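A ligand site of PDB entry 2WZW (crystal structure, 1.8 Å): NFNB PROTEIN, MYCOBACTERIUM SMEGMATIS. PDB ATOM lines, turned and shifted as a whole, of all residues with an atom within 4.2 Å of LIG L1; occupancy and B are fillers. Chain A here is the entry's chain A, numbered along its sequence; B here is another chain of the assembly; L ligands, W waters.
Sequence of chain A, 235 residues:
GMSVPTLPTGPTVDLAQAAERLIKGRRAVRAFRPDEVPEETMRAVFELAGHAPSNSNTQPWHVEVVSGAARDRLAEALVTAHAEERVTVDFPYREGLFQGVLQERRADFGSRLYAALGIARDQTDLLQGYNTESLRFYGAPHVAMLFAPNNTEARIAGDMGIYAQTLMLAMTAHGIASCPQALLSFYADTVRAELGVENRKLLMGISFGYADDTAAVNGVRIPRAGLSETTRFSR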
ATOM      1  N   VAL A  87      20.480  12.852   9.841  1.00  0.00           N
ATOM      2  CA  VAL A  87      20.735  11.420   9.890  1.00  0.00           C
ATOM      3  C   VAL A  87      20.884  10.922   8.432  1.00  0.00           C
ATOM      4  O   VAL A  87      20.045  11.237   7.589  1.00  0.00           O
ATOM      5  CB  VAL A  87      19.595  10.695  10.648  1.00  0.00           C
ATOM      6  CG1 VAL A  87      19.650   9.184  10.441  1.00  0.00           C
ATOM      7  CG2 VAL A  87      19.608  11.046  12.132  1.00  0.00           C
ATOM      8  N   TYR A  93      18.083   0.539  10.060  1.00  0.00           N
ATOM      9  CA  TYR A  93      17.944  -0.014  11.424  1.00  0.00           C
ATOM     10  C   TYR A  93      16.529   0.314  11.874  1.00  0.00           C
ATOM     11  O   TYR A  93      16.332   1.181  12.739  1.00  0.00           O
ATOM     12  CB  TYR A  93      18.991   0.620  12.360  1.00  0.00           C
ATOM     13  CG  TYR A  93      19.394  -0.150  13.595  1.00  0.00           C
ATOM     14  CD1 TYR A  93      20.714  -0.124  14.058  1.00  0.00           C
ATOM     15  CD2 TYR A  93      18.458  -0.844  14.363  1.00  0.00           C
ATOM     16  CE1 TYR A  93      21.096  -0.803  15.219  1.00  0.00           C
ATOM     17  CE2 TYR A  93      18.826  -1.539  15.514  1.00  0.00           C
ATOM     18  CZ  TYR A  93      20.150  -1.508  15.940  1.00  0.00           C
ATOM     19  OH  TYR A  93      20.520  -2.167  17.094  1.00  0.00           O
ATOM     20  N   GLN A 103      14.310  -9.083  21.223  1.00  0.00           N
ATOM     21  CA  GLN A 103      13.841  -7.803  21.757  1.00  0.00           C
ATOM     22  C   GLN A 103      14.011  -7.756  23.281  1.00  0.00           C
ATOM     23  O   GLN A 103      14.373  -6.695  23.820  1.00  0.00           O
ATOM     24  CB  GLN A 103      12.383  -7.502  21.318  1.00  0.00           C
ATOM     25  CG  GLN A 103      11.710  -6.266  21.964  1.00  0.00           C
ATOM     26  CD  GLN A 103      12.553  -4.989  22.034  1.00  0.00           C
ATOM     27  OE1 GLN A 103      13.420  -4.704  21.202  1.00  0.00           O
ATOM     28  NE2 GLN A 103      12.296  -4.175  23.066  1.00  0.00           N
ATOM     29  N   ARG A 106      17.624  -7.114  24.186  1.00  0.00           N
ATOM     30  CA  ARG A 106      17.876  -5.691  23.902  1.00  0.00           C
ATOM     31  C   ARG A 106      17.350  -4.812  25.075  1.00  0.00           C
ATOM     32  O   ARG A 106      18.067  -3.916  25.541  1.00  0.00           O
ATOM     33  CB  ARG A 106      17.221  -5.313  22.559  1.00  0.00           C
ATOM     34  CG  ARG A 106      17.190  -3.816  22.249  1.00  0.00           C
ATOM     35  CD  ARG A 106      16.889  -3.548  20.789  1.00  0.00           C
ATOM     36  NE  ARG A 106      16.742  -2.104  20.529  1.00  0.00           N
ATOM     37  CZ  ARG A 106      15.591  -1.446  20.552  1.00  0.00           C
ATOM     38  NH1 ARG A 106      14.458  -2.088  20.802  1.00  0.00           N
ATOM     39  NH2 ARG A 106      15.555  -0.147  20.297  1.00  0.00           N
ATOM     40  N   ALA A 107      16.118  -5.066  25.532  1.00  0.00           N
ATOM     41  CA  ALA A 107      15.503  -4.312  26.639  1.00  0.00           C
ATOM     42  C   ALA A 107      16.294  -4.519  27.941  1.00  0.00           C
ATOM     43  O   ALA A 107      16.513  -3.561  28.678  1.00  0.00           O
ATOM     44  CB  ALA A 107      14.053  -4.740  26.836  1.00  0.00           C
ATOM     45  N   GLY A 110      19.600  -2.580  27.824  1.00  0.00           N
ATOM     46  CA  GLY A 110      19.298  -1.166  27.994  1.00  0.00           C
ATOM     47  C   GLY A 110      19.047  -0.814  29.450  1.00  0.00           C
ATOM     48  O   GLY A 110      19.569   0.186  29.951  1.00  0.00           O
ATOM     49  N   SER A 111      18.269  -1.689  30.137  1.00  0.00           N
ATOM     50  CA  SER A 111      17.942  -1.500  31.550  1.00  0.00           C
ATOM     51  C   SER A 111      19.211  -1.500  32.403  1.00  0.00           C
ATOM     52  O   SER A 111      19.341  -0.671  33.297  1.00  0.00           O
ATOM     53  CB  SER A 111      16.966  -2.582  32.025  1.00  0.00           C
ATOM     54  OG  SER A 111      15.679  -2.345  31.477  1.00  0.00           O
ATOM     55  N   TYR A 114      21.436   1.874  31.172  1.00  0.00           N
ATOM     56  CA  TYR A 114      20.855   3.120  31.685  1.00  0.00           C
ATOM     57  C   TYR A 114      20.790   3.244  33.191  1.00  0.00           C
ATOM     58  O   TYR A 114      20.886   4.364  33.705  1.00  0.00           O
ATOM     59  CB  TYR A 114      19.586   3.533  30.939  1.00  0.00           C
ATOM     60  CG  TYR A 114      19.867   3.820  29.471  1.00  0.00           C
ATOM     61  CD1 TYR A 114      20.518   4.990  29.088  1.00  0.00           C
ATOM     62  CD2 TYR A 114      19.562   2.896  28.491  1.00  0.00           C
ATOM     63  CE1 TYR A 114      20.827   5.229  27.751  1.00  0.00           C
ATOM     64  CE2 TYR A 114      19.853   3.126  27.147  1.00  0.00           C
ATOM     65  CZ  TYR A 114      20.479   4.310  26.787  1.00  0.00           C
ATOM     66  OH  TYR A 114      20.762   4.552  25.463  1.00  0.00           O
ATOM     67  N   ILE A 119      20.343   7.213  34.242  1.00  0.00           N
ATOM     68  CA  ILE A 119      19.405   7.913  33.365  1.00  0.00           C
ATOM     69  C   ILE A 119      18.072   7.165  33.305  1.00  0.00           C
ATOM     70  O   ILE A 119      18.047   6.010  32.858  1.00  0.00           O
ATOM     71  CB  ILE A 119      19.994   8.167  31.945  1.00  0.00           C
ATOM     72  CG1 ILE A 119      21.343   8.929  32.029  1.00  0.00           C
ATOM     73  CG2 ILE A 119      18.985   8.916  31.058  1.00  0.00           C
ATOM     74  CD1 ILE A 119      22.186   8.938  30.739  1.00  0.00           C
ATOM     75  N   ALA A 120      16.982   7.830  33.737  1.00  0.00           N
ATOM     76  CA  ALA A 120      15.638   7.254  33.693  1.00  0.00           C
ATOM     77  C   ALA A 120      15.046   7.389  32.282  1.00  0.00           C
ATOM     78  O   ALA A 120      15.528   8.193  31.484  1.00  0.00           O
ATOM     79  CB  ALA A 120      14.739   7.944  34.719  1.00  0.00           C
ATOM     80  N   ARG A 121      14.003   6.597  31.964  1.00  0.00           N
ATOM     81  CA  ARG A 121      13.313   6.578  30.667  1.00  0.00           C
ATOM     82  C   ARG A 121      12.730   7.938  30.213  1.00  0.00           C
ATOM     83  O   ARG A 121      12.753   8.230  29.024  1.00  0.00           O
ATOM     84  CB  ARG A 121      12.214   5.497  30.648  1.00  0.00           C
ATOM     85  CG  ARG A 121      12.740   4.067  30.822  1.00  0.00           C
ATOM     86  CD  ARG A 121      11.618   3.049  30.766  1.00  0.00           C
ATOM     87  NE  ARG A 121      12.103   1.703  31.069  1.00  0.00           N
ATOM     88  CZ  ARG A 121      12.589   0.849  30.172  1.00  0.00           C
ATOM     89  NH1 ARG A 121      12.680   1.205  28.893  1.00  0.00           N
ATOM     90  NH2 ARG A 121      12.998  -0.358  30.537  1.00  0.00           N
ATOM     91  N   LEU A 127      19.404  11.987  28.254  1.00  0.00           N
ATOM     92  CA  LEU A 127      19.586  11.050  27.139  1.00  0.00           C
ATOM     93  C   LEU A 127      20.274  11.759  25.963  1.00  0.00           C
ATOM     94  O   LEU A 127      21.089  11.140  25.279  1.00  0.00           O
ATOM     95  CB  LEU A 127      18.251  10.417  26.695  1.00  0.00           C
ATOM     96  CG  LEU A 127      17.670   9.335  27.608  1.00  0.00           C
ATOM     97  CD1 LEU A 127      16.162   9.252  27.468  1.00  0.00           C
ATOM     98  CD2 LEU A 127      18.317   7.978  27.349  1.00  0.00           C
ATOM     99  N   ASN A 131      23.996  10.881  24.391  1.00  0.00           N
ATOM    100  CA  ASN A 131      24.174  10.650  22.954  1.00  0.00           C
ATOM    101  C   ASN A 131      25.221  11.572  22.338  1.00  0.00           C
ATOM    102  O   ASN A 131      25.938  11.145  21.428  1.00  0.00           O
ATOM    103  CB  ASN A 131      22.849  10.717  22.190  1.00  0.00           C
ATOM    104  CG  ASN A 131      21.981   9.496  22.403  1.00  0.00           C
ATOM    105  OD1 ASN A 131      22.371   8.348  22.131  1.00  0.00           O
ATOM    106  ND2 ASN A 131      20.766   9.723  22.886  1.00  0.00           N
ATOM    107  N   LEU A 183      25.869   3.519  16.328  1.00  0.00           N
ATOM    108  CA  LEU A 183      25.468   4.933  16.321  1.00  0.00           C
ATOM    109  C   LEU A 183      26.184   5.786  15.257  1.00  0.00           C
ATOM    110  O   LEU A 183      25.548   6.601  14.577  1.00  0.00           O
ATOM    111  CB  LEU A 183      25.641   5.566  17.710  1.00  0.00           C
ATOM    112  CG  LEU A 183      25.390   7.087  17.783  1.00  0.00           C
ATOM    113  CD1 LEU A 183      23.905   7.421  17.590  1.00  0.00           C
ATOM    114  CD2 LEU A 183      25.936   7.664  19.067  1.00  0.00           C
ATOM    115  N   PHE A 186      24.924   6.101  11.595  1.00  0.00           N
ATOM    116  CA  PHE A 186      23.716   6.894  11.316  1.00  0.00           C
ATOM    117  C   PHE A 186      24.052   8.287  10.769  1.00  0.00           C
ATOM    118  O   PHE A 186      23.133   9.065  10.465  1.00  0.00           O
ATOM    119  CB  PHE A 186      22.803   6.988  12.551  1.00  0.00           C
ATOM    120  CG  PHE A 186      22.080   5.676  12.749  1.00  0.00           C
ATOM    121  CD1 PHE A 186      20.814   5.478  12.211  1.00  0.00           C
ATOM    122  CD2 PHE A 186      22.711   4.607  13.377  1.00  0.00           C
ATOM    123  CE1 PHE A 186      20.169   4.242  12.335  1.00  0.00           C
ATOM    124  CE2 PHE A 186      22.057   3.374  13.511  1.00  0.00           C
ATOM    125  CZ  PHE A 186      20.798   3.205  13.003  1.00  0.00           C
ATOM    126  N   SER B  56      23.025  -4.354  20.801  1.00  0.00           N
ATOM    127  CA  SER B  56      22.122  -4.387  21.967  1.00  0.00           C
ATOM    128  C   SER B  56      22.153  -5.733  22.732  1.00  0.00           C
ATOM    129  O   SER B  56      21.150  -6.081  23.367  1.00  0.00           O
ATOM    130  CB  SER B  56      20.688  -4.140  21.515  1.00  0.00           C
ATOM    131  OG  SER B  56      20.471  -2.799  21.103  1.00  0.00           O
HETATM  132  P1  LIG L   1      19.485   2.003  22.621  1.00  0.00           P
HETATM  133  O1  LIG L   1      20.360   2.263  23.806  1.00  0.00           O
HETATM  134  O2  LIG L   1      18.847   3.152  21.905  1.00  0.00           O
HETATM  135  O3  LIG L   1      18.234   1.146  23.232  1.00  0.00           O
HETATM  136  C1  LIG L   1      18.519  -0.127  23.825  1.00  0.00           C
HETATM  137  C2  LIG L   1      17.367  -0.570  24.750  1.00  0.00           C
HETATM  138  O4  LIG L   1      17.335   0.295  25.899  1.00  0.00           O
HETATM  139  C3  LIG L   1      15.980  -0.484  24.092  1.00  0.00           C
HETATM  140  O5  LIG L   1      15.137  -1.582  24.561  1.00  0.00           O
HETATM  141  C4  LIG L   1      15.480   0.876  24.595  1.00  0.00           C
HETATM  142  O6  LIG L   1      14.076   0.990  24.458  1.00  0.00           O
HETATM  143  C5  LIG L   1      16.006   0.850  26.035  1.00  0.00           C
HETATM  144  N1  LIG L   1      16.172   2.103  26.755  1.00  0.00           N
HETATM  145  C6  LIG L   1      16.375   3.361  26.222  1.00  0.00           C
HETATM  146  N2  LIG L   1      16.490   4.298  27.165  1.00  0.00           N
HETATM  147  C7  LIG L   1      16.353   3.619  28.350  1.00  0.00           C
HETATM  148  C8  LIG L   1      16.388   4.015  29.723  1.00  0.00           C
HETATM  149  N3  LIG L   1      16.601   5.312  30.127  1.00  0.00           N
HETATM  150  N4  LIG L   1      16.222   3.054  30.711  1.00  0.00           N
HETATM  151  C9  LIG L   1      16.019   1.755  30.327  1.00  0.00           C
HETATM  152  N5  LIG L   1      15.980   1.267  29.054  1.00  0.00           N
HETATM  153  C10 LIG L   1      16.156   2.240  28.114  1.00  0.00           C
HETATM  154  O7  LIG L   1      20.107   0.922  21.603  1.00  0.00           O
HETATM  155  P2  LIG L   1      19.587   0.482  20.138  1.00  0.00           P
HETATM  156  O8  LIG L   1      20.182  -0.802  19.618  1.00  0.00           O
HETATM  157  O9  LIG L   1      18.086   0.759  20.065  1.00  0.00           O
HETATM  158  O10 LIG L   1      20.252   1.641  19.218  1.00  0.00           O
HETATM  159  C11 LIG L   1      21.605   1.515  18.785  1.00  0.00           C
HETATM  160  C12 LIG L   1      22.405   2.822  18.685  1.00  0.00           C
HETATM  161  O11 LIG L   1      22.143   3.315  17.366  1.00  0.00           O
HETATM  162  C13 LIG L   1      21.994   3.950  19.656  1.00  0.00           C
HETATM  163  O12 LIG L   1      23.045   4.894  19.884  1.00  0.00           O
HETATM  164  C14 LIG L   1      20.793   4.566  18.966  1.00  0.00           C
HETATM  165  O13 LIG L   1      20.584   5.935  19.390  1.00  0.00           O
HETATM  166  C15 LIG L   1      21.198   4.426  17.485  1.00  0.00           C
HETATM  167  N6  LIG L   1      20.040   4.254  16.585  1.00  0.00           N
HETATM  168  C16 LIG L   1      19.589   5.379  15.836  1.00  0.00           C
HETATM  169  C17 LIG L   1      18.531   5.329  14.962  1.00  0.00           C
HETATM  170  C18 LIG L   1      18.136   6.581  14.196  1.00  0.00           C
HETATM  171  O14 LIG L   1      18.726   7.675  14.316  1.00  0.00           O
HETATM  172  N7  LIG L   1      17.077   6.477  13.335  1.00  0.00           N
HETATM  173  C19 LIG L   1      17.776   4.002  14.779  1.00  0.00           C
HETATM  174  C20 LIG L   1      18.306   2.840  15.615  1.00  0.00           C
HETATM  175  C21 LIG L   1      19.363   3.017  16.445  1.00  0.00           C
HETATM  176  P3  LIG L   1      13.467   1.829  23.204  1.00  0.00           P
HETATM  177  O15 LIG L   1      12.803   0.844  22.269  1.00  0.00           O
HETATM  178  O16 LIG L   1      12.472   2.665  23.969  1.00  0.00           O
HETATM  179  O17 LIG L   1      14.531   2.639  22.492  1.00  0.00           O
HETATM  180  N1  LG2 L   2      27.078   0.110  22.266  1.00  0.00           N
HETATM  181  C1  LG2 L   2      26.820   1.437  22.351  1.00  0.00           C
HETATM  182  O1  LG2 L   2      26.909   2.031  23.556  1.00  0.00           O
HETATM  183  N2  LG2 L   2      26.484   2.163  21.263  1.00  0.00           N
HETATM  184  C2  LG2 L   2      26.365   1.562  20.061  1.00  0.00           C
HETATM  185  O2  LG2 L   2      26.019   2.277  18.986  1.00  0.00           O
HETATM  186  C3  LG2 L   2      26.626   0.189  19.940  1.00  0.00           C
HETATM  187  N3  LG2 L   2      26.515  -0.465  18.698  1.00  0.00           N
HETATM  188  C4  LG2 L   2      27.060  -1.761  18.565  1.00  0.00           C
HETATM  189  C5  LG2 L   2      27.247  -2.323  17.291  1.00  0.00           C
HETATM  190  C6  LG2 L   2      27.777  -3.608  17.171  1.00  0.00           C
HETATM  191  C7  LG2 L   2      27.950  -4.243  15.780  1.00  0.00           C
HETATM  192  C8  LG2 L   2      28.161  -4.319  18.322  1.00  0.00           C
HETATM  193  C9  LG2 L   2      28.793  -5.719  18.210  1.00  0.00           C
HETATM  194  C10 LG2 L   2      27.977  -3.761  19.580  1.00  0.00           C
HETATM  195  C11 LG2 L   2      27.466  -2.467  19.706  1.00  0.00           C
HETATM  196  N4  LG2 L   2      27.307  -1.885  21.004  1.00  0.00           N
HETATM  197  C12 LG2 L   2      26.991  -0.530  21.085  1.00  0.00           C
HETATM  198  C13 LG2 L   2      27.949  -2.543  22.193  1.00  0.00           C
HETATM  199  C14 LG2 L   2      26.979  -3.441  22.989  1.00  0.00           C
HETATM  200  O3  LG2 L   2      25.804  -3.103  23.191  1.00  0.00           O
HETATM  201  C15 LG2 L   2      27.592  -4.673  23.662  1.00  0.00           C
HETATM  202  O4  LG2 L   2      28.600  -5.338  22.856  1.00  0.00           O
HETATM  203  C16 LG2 L   2      26.567  -5.673  24.229  1.00  0.00           C
HETATM  204  O5  LG2 L   2      25.737  -4.973  25.180  1.00  0.00           O
HETATM  205  C17 LG2 L   2      27.339  -6.769  24.982  1.00  0.00           C
HETATM  206  O6  LG2 L   2      28.096  -6.161  26.074  1.00  0.00           O
HETATM  207  P1  LG2 L   2      29.689  -6.316  26.196  1.00  0.00           P
HETATM  208  O7  LG2 L   2      30.370  -6.009  24.784  1.00  0.00           O
HETATM  209  O8  LG2 L   2      30.146  -5.193  27.216  1.00  0.00           O
HETATM  210  O9  LG2 L   2      30.080  -7.686  26.636  1.00  0.00           O
HETATM  211  O   HOH W   1      16.439   3.415  20.755  1.00  0.00           O
HETATM  212  O   HOH W   2      14.982  -1.334  28.675  1.00  0.00           O
HETATM  213  O   HOH W   3      16.546   3.230  33.591  1.00  0.00           O
HETATM  214  O   HOH W   4      24.614   5.412  21.987  1.00  0.00           O
HETATM  215  O   HOH W   5      20.720   8.928  15.955  1.00  0.00           O
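Water W2 lies within hydrogen-bond range of O of Ala 107 (2.7 Å), N5 of LIG L1 (2.8 Å), NH2 of Arg 121 (2.9 Å) and OG of Ser 111 (3.1 Å).
Water W3 lies within hydrogen-bond range of N4 of LIG L1 (2.9 Å) and O of Ile 119 (3.2 Å).
The guanidinium group (NH2) of Arg 106 is in salt-bridge range of an oxygen (O9) of LIG L1 (2.7 Å).
NH1 of Arg 121 is in hydrogen-bond range of N5 of LIG L1 (3.3 Å).
The side-chain hydroxyl of Tyr 114 is in hydrogen-bond range of an oxygen (O1) of LIG L1 (2.9 Å).
An oxygen (O2) of LG2 L2 sits at hydrogen-bond distance from the backbone NH (N) of Leu 183.
The side-chain hydroxyl (OH) of Tyr 93 is in hydrogen-bond range of an oxygen (O8) of LIG L1 (2.9 Å).
O of Ile 119 is in hydrogen-bond range of N3 of LIG L1, at 3.2 Å.
OG of Ser 56 of chain B sits at hydrogen-bond distance from O8 of LIG L1, at 2.5 Å.
N3 of LIG L1 sits at hydrogen-bond distance from O of Ala 120 (3.4 Å).
The side-chain amide oxygen of Gln 103 sits at hydrogen-bond distance from the guanidinium group of Arg 106, 2.8 Å away.
The backbone carbonyl oxygen (O) of Ala 107 is in hydrogen-bond range of the side-chain hydroxyl (OG) of Ser 111 (3.2 Å).
N of Ile 119 sits at hydrogen-bond distance from O of Tyr 114 (2.9 Å).
The side-chain hydroxyl (OG) of Ser 111 is in hydrogen-bond range of the guanidinium group (NH2) of Arg 121.
Residues that only touch LIG L1: Gly 110 (3.2 Å), Phe 186 (3.3 Å), Ala 107 (3.5 Å), Leu 183 (3.5 Å) and Ser 111 (3.9 Å).
Within 4 Å of LIG L1: Tyr 93, Arg 106, Ala 107, Gly 110, Ser 111, Tyr 114, Ile 119, Ala 120, Arg 121, Leu 183, Phe 186 and Ser 56 of chain B.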
